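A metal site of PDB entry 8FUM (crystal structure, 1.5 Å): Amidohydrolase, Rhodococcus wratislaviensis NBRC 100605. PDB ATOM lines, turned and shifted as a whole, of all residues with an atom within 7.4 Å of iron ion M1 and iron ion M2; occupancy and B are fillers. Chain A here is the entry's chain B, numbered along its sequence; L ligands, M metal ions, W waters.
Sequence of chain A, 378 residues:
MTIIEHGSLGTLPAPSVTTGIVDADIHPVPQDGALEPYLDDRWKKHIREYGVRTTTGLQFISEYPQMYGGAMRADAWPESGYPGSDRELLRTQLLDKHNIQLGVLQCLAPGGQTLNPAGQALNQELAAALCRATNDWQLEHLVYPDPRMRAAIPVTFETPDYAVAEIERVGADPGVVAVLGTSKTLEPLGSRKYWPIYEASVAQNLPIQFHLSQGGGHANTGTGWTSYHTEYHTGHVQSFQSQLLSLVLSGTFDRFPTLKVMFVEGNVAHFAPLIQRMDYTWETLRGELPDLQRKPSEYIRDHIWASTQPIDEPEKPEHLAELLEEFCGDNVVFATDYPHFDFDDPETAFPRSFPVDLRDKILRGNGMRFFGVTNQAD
The side-chain carboxylate (OD2) of Asp 337 lies close to the side-chain amide nitrogen (NE2) of Gln 309 (3.3 Å). The backbone NH (N) of His 27 is in hydrogen-bond range of the backbone carbonyl oxygen (O) of Tyr 338, at 2.9 Å. The side-chain carboxylate (OD1) of Asp 25 lies close to the side-chain amide oxygen (OE1) of Gln 106. The side-chain amide oxygen (OE1) of Gln 309 sits close to the side-chain carboxylate (OE1) of Glu 265 (3.3 Å). A ring nitrogen (ND1) of His 27 lies within hydrogen-bond range of the backbone carbonyl oxygen (O) of Gln 106 (2.7 Å).
Within 4 Å of iron ion M1: Asp 25, His 27, His 211, Glu 265 and Asp 337. The nearest printed residue that does not touch iron ion M1 is His 340 (4.3 Å).
Three residues have an atom within 4 Å of iron ion M2: Glu 265, Asp 337 and His 340. The nearest printed residue that does not touch iron ion M2 is Asp 342 (4.3 Å).
Iron ion M1 is bound by water W1, the side-chain carboxylate of Glu 265, the side-chain carboxylate of Asp 337, a ring nitrogen (NE2) of His 27, the side-chain carboxylate of Asp 25 and a ring nitrogen (NE2) of His 211. Iron ion M1 has six donor atoms within binding distance.
Iron ion M2 is bound by water W1 (2.1 Å), the side-chain carboxylate (OD2) of Asp 337 (2.1 Å), the side-chain carboxylate (OE2) of Glu 265 (2.1 Å), an oxygen (O1) of the ligand (2.2 Å), a nitrogen (N1) of the ligand (2.2 Å) and a ring nitrogen (ND1) of His 340 (2.2 Å).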
ATOM      1  N   ASP A  25      -3.962   9.830 -22.782  1.00  0.00           N
ATOM      2  CA  ASP A  25      -4.096  10.374 -21.413  1.00  0.00           C
ATOM      3  C   ASP A  25      -4.615  11.817 -21.480  1.00  0.00           C
ATOM      4  O   ASP A  25      -3.835  12.751 -21.713  1.00  0.00           O
ATOM      5  CB  ASP A  25      -2.789  10.285 -20.637  1.00  0.00           C
ATOM      6  CG  ASP A  25      -2.960  10.581 -19.150  1.00  0.00           C
ATOM      7  OD1 ASP A  25      -4.065  10.322 -18.613  1.00  0.00           O
ATOM      8  OD2 ASP A  25      -1.994  11.034 -18.507  1.00  0.00           O
ATOM      9  N   ILE A  26      -5.911  11.971 -21.214  1.00  0.00           N
ATOM     10  CA  ILE A  26      -6.586  13.255 -21.113  1.00  0.00           C
ATOM     11  C   ILE A  26      -7.301  13.288 -19.773  1.00  0.00           C
ATOM     12  O   ILE A  26      -7.902  12.294 -19.374  1.00  0.00           O
ATOM     13  CB  ILE A  26      -7.627  13.381 -22.254  1.00  0.00           C
ATOM     14  CG1 ILE A  26      -6.915  13.304 -23.601  1.00  0.00           C
ATOM     15  CG2 ILE A  26      -8.435  14.676 -22.108  1.00  0.00           C
ATOM     16  CD1 ILE A  26      -7.901  13.071 -24.764  1.00  0.00           C
ATOM     17  N   HIS A  27      -7.288  14.443 -19.108  1.00  0.00           N
ATOM     18  CA  HIS A  27      -7.838  14.565 -17.753  1.00  0.00           C
ATOM     19  C   HIS A  27      -9.016  15.520 -17.700  1.00  0.00           C
ATOM     20  O   HIS A  27      -8.839  16.717 -17.470  1.00  0.00           O
ATOM     21  CB  HIS A  27      -6.746  14.998 -16.777  1.00  0.00           C
ATOM     22  CG  HIS A  27      -5.631  14.013 -16.709  1.00  0.00           C
ATOM     23  ND1 HIS A  27      -5.856  12.682 -16.403  1.00  0.00           N
ATOM     24  CD2 HIS A  27      -4.305  14.122 -16.942  1.00  0.00           C
ATOM     25  CE1 HIS A  27      -4.721  12.024 -16.444  1.00  0.00           C
ATOM     26  NE2 HIS A  27      -3.759  12.866 -16.788  1.00  0.00           N
ATOM     27  N   ALA A  71      -0.425  22.772 -11.282  1.00  0.00           N
ATOM     28  CA  ALA A  71       0.197  21.924 -12.282  1.00  0.00           C
ATOM     29  C   ALA A  71      -0.581  21.912 -13.594  1.00  0.00           C
ATOM     30  O   ALA A  71      -0.488  20.959 -14.359  1.00  0.00           O
ATOM     31  CB  ALA A  71       0.421  20.492 -11.764  1.00  0.00           C
ATOM     32  N   GLN A 106      -8.961   9.834 -18.500  1.00  0.00           N
ATOM     33  CA  GLN A 106      -8.502   9.298 -17.222  1.00  0.00           C
ATOM     34  C   GLN A 106      -8.890  10.325 -16.161  1.00  0.00           C
ATOM     35  O   GLN A 106      -8.190  11.316 -15.948  1.00  0.00           O
ATOM     36  CB  GLN A 106      -7.015   9.024 -17.258  1.00  0.00           C
ATOM     37  CG  GLN A 106      -6.638   8.095 -18.398  1.00  0.00           C
ATOM     38  CD  GLN A 106      -5.266   7.494 -18.281  1.00  0.00           C
ATOM     39  OE1 GLN A 106      -4.695   7.410 -17.181  1.00  0.00           O
ATOM     40  NE2 GLN A 106      -4.725   7.050 -19.397  1.00  0.00           N
ATOM     41  N   LEU A 108      -9.021  11.734 -12.761  1.00  0.00           N
ATOM     42  CA  LEU A 108      -8.162  11.564 -11.600  1.00  0.00           C
ATOM     43  C   LEU A 108      -8.709  12.194 -10.328  1.00  0.00           C
ATOM     44  O   LEU A 108      -8.015  12.161  -9.313  1.00  0.00           O
ATOM     45  CB  LEU A 108      -6.802  12.208 -11.866  1.00  0.00           C
ATOM     46  CG  LEU A 108      -5.997  11.735 -13.079  1.00  0.00           C
ATOM     47  CD1 LEU A 108      -4.761  12.623 -13.179  1.00  0.00           C
ATOM     48  CD2 LEU A 108      -5.660  10.252 -12.921  1.00  0.00           C
ATOM     49  N   THR A 114      -6.543  18.312  -9.196  1.00  0.00           N
ATOM     50  CA  THR A 114      -5.648  17.730 -10.192  1.00  0.00           C
ATOM     51  C   THR A 114      -5.431  16.232 -10.035  1.00  0.00           C
ATOM     52  O   THR A 114      -5.453  15.503 -11.032  1.00  0.00           O
ATOM     53  CB  THR A 114      -4.315  18.463 -10.131  1.00  0.00           C
ATOM     54  OG1 THR A 114      -4.513  19.851 -10.474  1.00  0.00           O
ATOM     55  CG2 THR A 114      -3.314  17.823 -11.071  1.00  0.00           C
ATOM     56  N   LEU A 115      -5.209  15.743  -8.814  1.00  0.00           N
ATOM     57  CA  LEU A 115      -4.861  14.327  -8.631  1.00  0.00           C
ATOM     58  C   LEU A 115      -5.351  13.914  -7.238  1.00  0.00           C
ATOM     59  O   LEU A 115      -4.651  14.131  -6.250  1.00  0.00           O
ATOM     60  CB  LEU A 115      -3.362  14.120  -8.778  1.00  0.00           C
ATOM     61  CG  LEU A 115      -2.763  12.738  -8.548  1.00  0.00           C
ATOM     62  CD1 LEU A 115      -3.308  11.685  -9.493  1.00  0.00           C
ATOM     63  CD2 LEU A 115      -1.235  12.791  -8.648  1.00  0.00           C
ATOM     64  N   HIS A 211      -2.218   4.812 -14.262  1.00  0.00           N
ATOM     65  CA  HIS A 211      -1.769   6.196 -14.319  1.00  0.00           C
ATOM     66  C   HIS A 211      -1.013   6.568 -13.055  1.00  0.00           C
ATOM     67  O   HIS A 211      -1.360   6.134 -11.950  1.00  0.00           O
ATOM     68  CB  HIS A 211      -2.957   7.145 -14.481  1.00  0.00           C
ATOM     69  CG  HIS A 211      -2.568   8.568 -14.751  1.00  0.00           C
ATOM     70  ND1 HIS A 211      -2.148   9.427 -13.756  1.00  0.00           N
ATOM     71  CD2 HIS A 211      -2.541   9.281 -15.897  1.00  0.00           C
ATOM     72  CE1 HIS A 211      -1.886  10.603 -14.284  1.00  0.00           C
ATOM     73  NE2 HIS A 211      -2.102  10.548 -15.585  1.00  0.00           N
ATOM     74  N   LEU A 212       0.032   7.379 -13.235  1.00  0.00           N
ATOM     75  CA  LEU A 212       0.738   7.984 -12.111  1.00  0.00           C
ATOM     76  C   LEU A 212      -0.202   8.363 -10.977  1.00  0.00           C
ATOM     77  O   LEU A 212      -1.274   8.946 -11.194  1.00  0.00           O
ATOM     78  CB  LEU A 212       1.476   9.209 -12.662  1.00  0.00           C
ATOM     79  CG  LEU A 212       2.072  10.353 -11.866  1.00  0.00           C
ATOM     80  CD1 LEU A 212       2.910  11.119 -12.873  1.00  0.00           C
ATOM     81  CD2 LEU A 212       1.020  11.257 -11.247  1.00  0.00           C
ATOM     82  N   HIS A 233       8.386  14.568  -8.343  1.00  0.00           N
ATOM     83  CA  HIS A 233       7.901  14.389  -9.699  1.00  0.00           C
ATOM     84  C   HIS A 233       8.770  13.400 -10.455  1.00  0.00           C
ATOM     85  O   HIS A 233       8.262  12.437 -11.062  1.00  0.00           O
ATOM     86  CB  HIS A 233       7.808  15.765 -10.353  1.00  0.00           C
ATOM     87  CG  HIS A 233       7.003  15.770 -11.622  1.00  0.00           C
ATOM     88  ND1 HIS A 233       6.580  16.938 -12.210  1.00  0.00           N
ATOM     89  CD2 HIS A 233       6.524  14.764 -12.391  1.00  0.00           C
ATOM     90  CE1 HIS A 233       5.902  16.651 -13.314  1.00  0.00           C
ATOM     91  NE2 HIS A 233       5.865  15.335 -13.453  1.00  0.00           N
ATOM     92  N   VAL A 264       1.087   4.583 -17.719  1.00  0.00           N
ATOM     93  CA  VAL A 264       0.759   5.921 -18.198  1.00  0.00           C
ATOM     94  C   VAL A 264       1.416   6.963 -17.306  1.00  0.00           C
ATOM     95  O   VAL A 264       1.146   7.037 -16.101  1.00  0.00           O
ATOM     96  CB  VAL A 264      -0.757   6.131 -18.259  1.00  0.00           C
ATOM     97  CG1 VAL A 264      -1.086   7.569 -18.660  1.00  0.00           C
ATOM     98  CG2 VAL A 264      -1.400   5.100 -19.199  1.00  0.00           C
ATOM     99  N   GLU A 265       2.288   7.777 -17.897  1.00  0.00           N
ATOM    100  CA  GLU A 265       2.947   8.886 -17.238  1.00  0.00           C
ATOM    101  C   GLU A 265       4.003   8.405 -16.248  1.00  0.00           C
ATOM    102  O   GLU A 265       4.344   9.116 -15.293  1.00  0.00           O
ATOM    103  CB  GLU A 265       1.963   9.872 -16.603  1.00  0.00           C
ATOM    104  CG  GLU A 265       2.476  11.298 -16.543  1.00  0.00           C
ATOM    105  CD  GLU A 265       1.365  12.296 -16.422  1.00  0.00           C
ATOM    106  OE1 GLU A 265       0.244  11.957 -16.914  1.00  0.00           O
ATOM    107  OE2 GLU A 265       1.581  13.394 -15.847  1.00  0.00           O
ATOM    108  N   GLN A 309       4.097  10.773 -22.629  1.00  0.00           N
ATOM    109  CA  GLN A 309       4.208  12.041 -21.928  1.00  0.00           C
ATOM    110  C   GLN A 309       4.621  11.798 -20.473  1.00  0.00           C
ATOM    111  O   GLN A 309       4.173  10.831 -19.853  1.00  0.00           O
ATOM    112  CB  GLN A 309       2.859  12.782 -21.986  1.00  0.00           C
ATOM    113  CG  GLN A 309       2.784  14.156 -21.344  1.00  0.00           C
ATOM    114  CD  GLN A 309       2.688  14.126 -19.843  1.00  0.00           C
ATOM    115  OE1 GLN A 309       2.296  13.137 -19.245  1.00  0.00           O
ATOM    116  NE2 GLN A 309       2.998  15.257 -19.237  1.00  0.00           N
ATOM    117  N   PRO A 310       5.471  12.643 -19.893  1.00  0.00           N
ATOM    118  CA  PRO A 310       6.203  13.747 -20.519  1.00  0.00           C
ATOM    119  C   PRO A 310       7.400  13.167 -21.247  1.00  0.00           C
ATOM    120  O   PRO A 310       8.194  12.410 -20.677  1.00  0.00           O
ATOM    121  CB  PRO A 310       6.617  14.592 -19.341  1.00  0.00           C
ATOM    122  CG  PRO A 310       6.778  13.609 -18.195  1.00  0.00           C
ATOM    123  CD  PRO A 310       5.733  12.553 -18.438  1.00  0.00           C
ATOM    124  N   ALA A 335       0.544  10.358 -25.795  1.00  0.00           N
ATOM    125  CA  ALA A 335      -0.400  11.046 -24.937  1.00  0.00           C
ATOM    126  C   ALA A 335       0.002  12.519 -24.848  1.00  0.00           C
ATOM    127  O   ALA A 335       1.189  12.857 -24.889  1.00  0.00           O
ATOM    128  CB  ALA A 335      -0.373  10.444 -23.521  1.00  0.00           C
ATOM    129  N   THR A 336      -1.001  13.369 -24.635  1.00  0.00           N
ATOM    130  CA  THR A 336      -0.755  14.782 -24.384  1.00  0.00           C
ATOM    131  C   THR A 336      -0.695  15.149 -22.909  1.00  0.00           C
ATOM    132  O   THR A 336       0.050  16.056 -22.548  1.00  0.00           O
ATOM    133  CB  THR A 336      -1.820  15.709 -25.016  1.00  0.00           C
ATOM    134  OG1 THR A 336      -3.090  15.524 -24.384  1.00  0.00           O
ATOM    135  CG2 THR A 336      -1.917  15.523 -26.523  1.00  0.00           C
ATOM    136  N   ASP A 337      -1.472  14.474 -22.065  1.00  0.00           N
ATOM    137  CA  ASP A 337      -1.697  14.864 -20.681  1.00  0.00           C
ATOM    138  C   ASP A 337      -2.456  16.182 -20.536  1.00  0.00           C
ATOM    139  O   ASP A 337      -2.347  16.856 -19.507  1.00  0.00           O
ATOM    140  CB  ASP A 337      -0.395  14.923 -19.884  1.00  0.00           C
ATOM    141  CG  ASP A 337      -0.608  14.658 -18.417  1.00  0.00           C
ATOM    142  OD1 ASP A 337      -1.532  13.869 -18.105  1.00  0.00           O
ATOM    143  OD2 ASP A 337       0.142  15.230 -17.589  1.00  0.00           O
ATOM    144  N   TYR A 338      -3.222  16.582 -21.543  1.00  0.00           N
ATOM    145  CA  TYR A 338      -4.029  17.781 -21.404  1.00  0.00           C
ATOM    146  C   TYR A 338      -4.918  17.662 -20.169  1.00  0.00           C
ATOM    147  O   TYR A 338      -5.571  16.630 -19.992  1.00  0.00           O
ATOM    148  CB  TYR A 338      -4.923  17.906 -22.638  1.00  0.00           C
ATOM    149  CG  TYR A 338      -5.790  19.143 -22.612  1.00  0.00           C
ATOM    150  CD1 TYR A 338      -5.308  20.355 -23.100  1.00  0.00           C
ATOM    151  CD2 TYR A 338      -7.076  19.107 -22.080  1.00  0.00           C
ATOM    152  CE1 TYR A 338      -6.088  21.507 -23.045  1.00  0.00           C
ATOM    153  CE2 TYR A 338      -7.863  20.234 -22.044  1.00  0.00           C
ATOM    154  CZ  TYR A 338      -7.362  21.438 -22.518  1.00  0.00           C
ATOM    155  OH  TYR A 338      -8.152  22.558 -22.476  1.00  0.00           O
ATOM    156  N   PRO A 339      -5.042  18.718 -19.332  1.00  0.00           N
ATOM    157  CA  PRO A 339      -4.460  20.057 -19.460  1.00  0.00           C
ATOM    158  C   PRO A 339      -3.287  20.346 -18.536  1.00  0.00           C
ATOM    159  O   PRO A 339      -3.105  21.497 -18.127  1.00  0.00           O
ATOM    160  CB  PRO A 339      -5.646  20.961 -19.085  1.00  0.00           C
ATOM    161  CG  PRO A 339      -6.440  20.138 -18.084  1.00  0.00           C
ATOM    162  CD  PRO A 339      -5.998  18.679 -18.225  1.00  0.00           C
ATOM    163  N   HIS A 340      -2.475  19.340 -18.217  1.00  0.00           N
ATOM    164  CA  HIS A 340      -1.410  19.551 -17.253  1.00  0.00           C
ATOM    165  C   HIS A 340      -0.266  20.365 -17.863  1.00  0.00           C
ATOM    166  O   HIS A 340      -0.098  20.430 -19.083  1.00  0.00           O
ATOM    167  CB  HIS A 340      -0.895  18.211 -16.713  1.00  0.00           C
ATOM    168  CG  HIS A 340      -1.915  17.496 -15.888  1.00  0.00           C
ATOM    169  ND1 HIS A 340      -1.663  16.286 -15.272  1.00  0.00           N
ATOM    170  CD2 HIS A 340      -3.187  17.828 -15.566  1.00  0.00           C
ATOM    171  CE1 HIS A 340      -2.747  15.898 -14.624  1.00  0.00           C
ATOM    172  NE2 HIS A 340      -3.679  16.828 -14.753  1.00  0.00           N
ATOM    173  N   PHE A 341       0.520  20.984 -16.977  1.00  0.00           N
ATOM    174  CA  PHE A 341       1.500  21.983 -17.397  1.00  0.00           C
ATOM    175  C   PHE A 341       2.560  21.395 -18.312  1.00  0.00           C
ATOM    176  O   PHE A 341       3.108  22.108 -19.172  1.00  0.00           O
ATOM    177  CB  PHE A 341       2.155  22.662 -16.165  1.00  0.00           C
ATOM    178  CG  PHE A 341       3.309  21.885 -15.571  1.00  0.00           C
ATOM    179  CD1 PHE A 341       3.076  20.875 -14.645  1.00  0.00           C
ATOM    180  CD2 PHE A 341       4.618  22.165 -15.943  1.00  0.00           C
ATOM    181  CE1 PHE A 341       4.146  20.163 -14.103  1.00  0.00           C
ATOM    182  CE2 PHE A 341       5.672  21.467 -15.408  1.00  0.00           C
ATOM    183  CZ  PHE A 341       5.441  20.465 -14.488  1.00  0.00           C
ATOM    184  N   ASP A 342       2.911  20.122 -18.130  1.00  0.00           N
ATOM    185  CA  ASP A 342       3.907  19.465 -18.959  1.00  0.00           C
ATOM    186  C   ASP A 342       3.292  18.714 -20.149  1.00  0.00           C
ATOM    187  O   ASP A 342       3.888  17.766 -20.678  1.00  0.00           O
ATOM    188  CB  ASP A 342       4.860  18.591 -18.118  1.00  0.00           C
ATOM    189  CG  ASP A 342       4.133  17.542 -17.247  1.00  0.00           C
ATOM    190  OD1 ASP A 342       2.888  17.555 -17.179  1.00  0.00           O
ATOM    191  OD2 ASP A 342       4.845  16.694 -16.645  1.00  0.00           O
ATOM    192  N   PHE A 343       2.106  19.162 -20.557  1.00  0.00           N
ATOM    193  CA  PHE A 343       1.474  18.787 -21.807  1.00  0.00           C
ATOM    194  C   PHE A 343       2.489  18.647 -22.938  1.00  0.00           C
ATOM    195  O   PHE A 343       3.376  19.491 -23.108  1.00  0.00           O
ATOM    196  CB  PHE A 343       0.504  19.921 -22.145  1.00  0.00           C
ATOM    197  CG  PHE A 343      -0.118  19.841 -23.516  1.00  0.00           C
ATOM    198  CD1 PHE A 343      -1.286  19.127 -23.737  1.00  0.00           C
ATOM    199  CD2 PHE A 343       0.460  20.509 -24.574  1.00  0.00           C
ATOM    200  CE1 PHE A 343      -1.850  19.064 -25.009  1.00  0.00           C
ATOM    201  CE2 PHE A 343      -0.094  20.447 -25.823  1.00  0.00           C
ATOM    202  CZ  PHE A 343      -1.252  19.730 -26.044  1.00  0.00           C
HETATM  203  C1  LIG L   1       1.407  15.847 -12.918  1.00  0.00           C
HETATM  204  C2  LIG L   1       2.206  16.517 -14.048  1.00  0.00           C
HETATM  205  C3  LIG L   1       0.316  16.792 -12.381  1.00  0.00           C
HETATM  206  C4  LIG L   1       2.388  15.432 -11.822  1.00  0.00           C
HETATM  207  N1  LIG L   1       0.730  14.656 -13.417  1.00  0.00           N
HETATM  208  O1  LIG L   1       1.488  16.433 -15.260  1.00  0.00           O
HETATM  209  O2  LIG L   1      -0.508  16.070 -11.481  1.00  0.00           O
HETATM  210  O3  LIG L   1       3.031  16.587 -11.315  1.00  0.00           O
HETATM  211 FE    FE M   1      -1.752  12.281 -16.842  1.00  0.00          FE
HETATM  212 FE    FE M   2       0.012  14.810 -15.525  1.00  0.00          FE
HETATM  213  O   HOH W   1      -1.393  13.329 -15.235  1.00  0.00           O
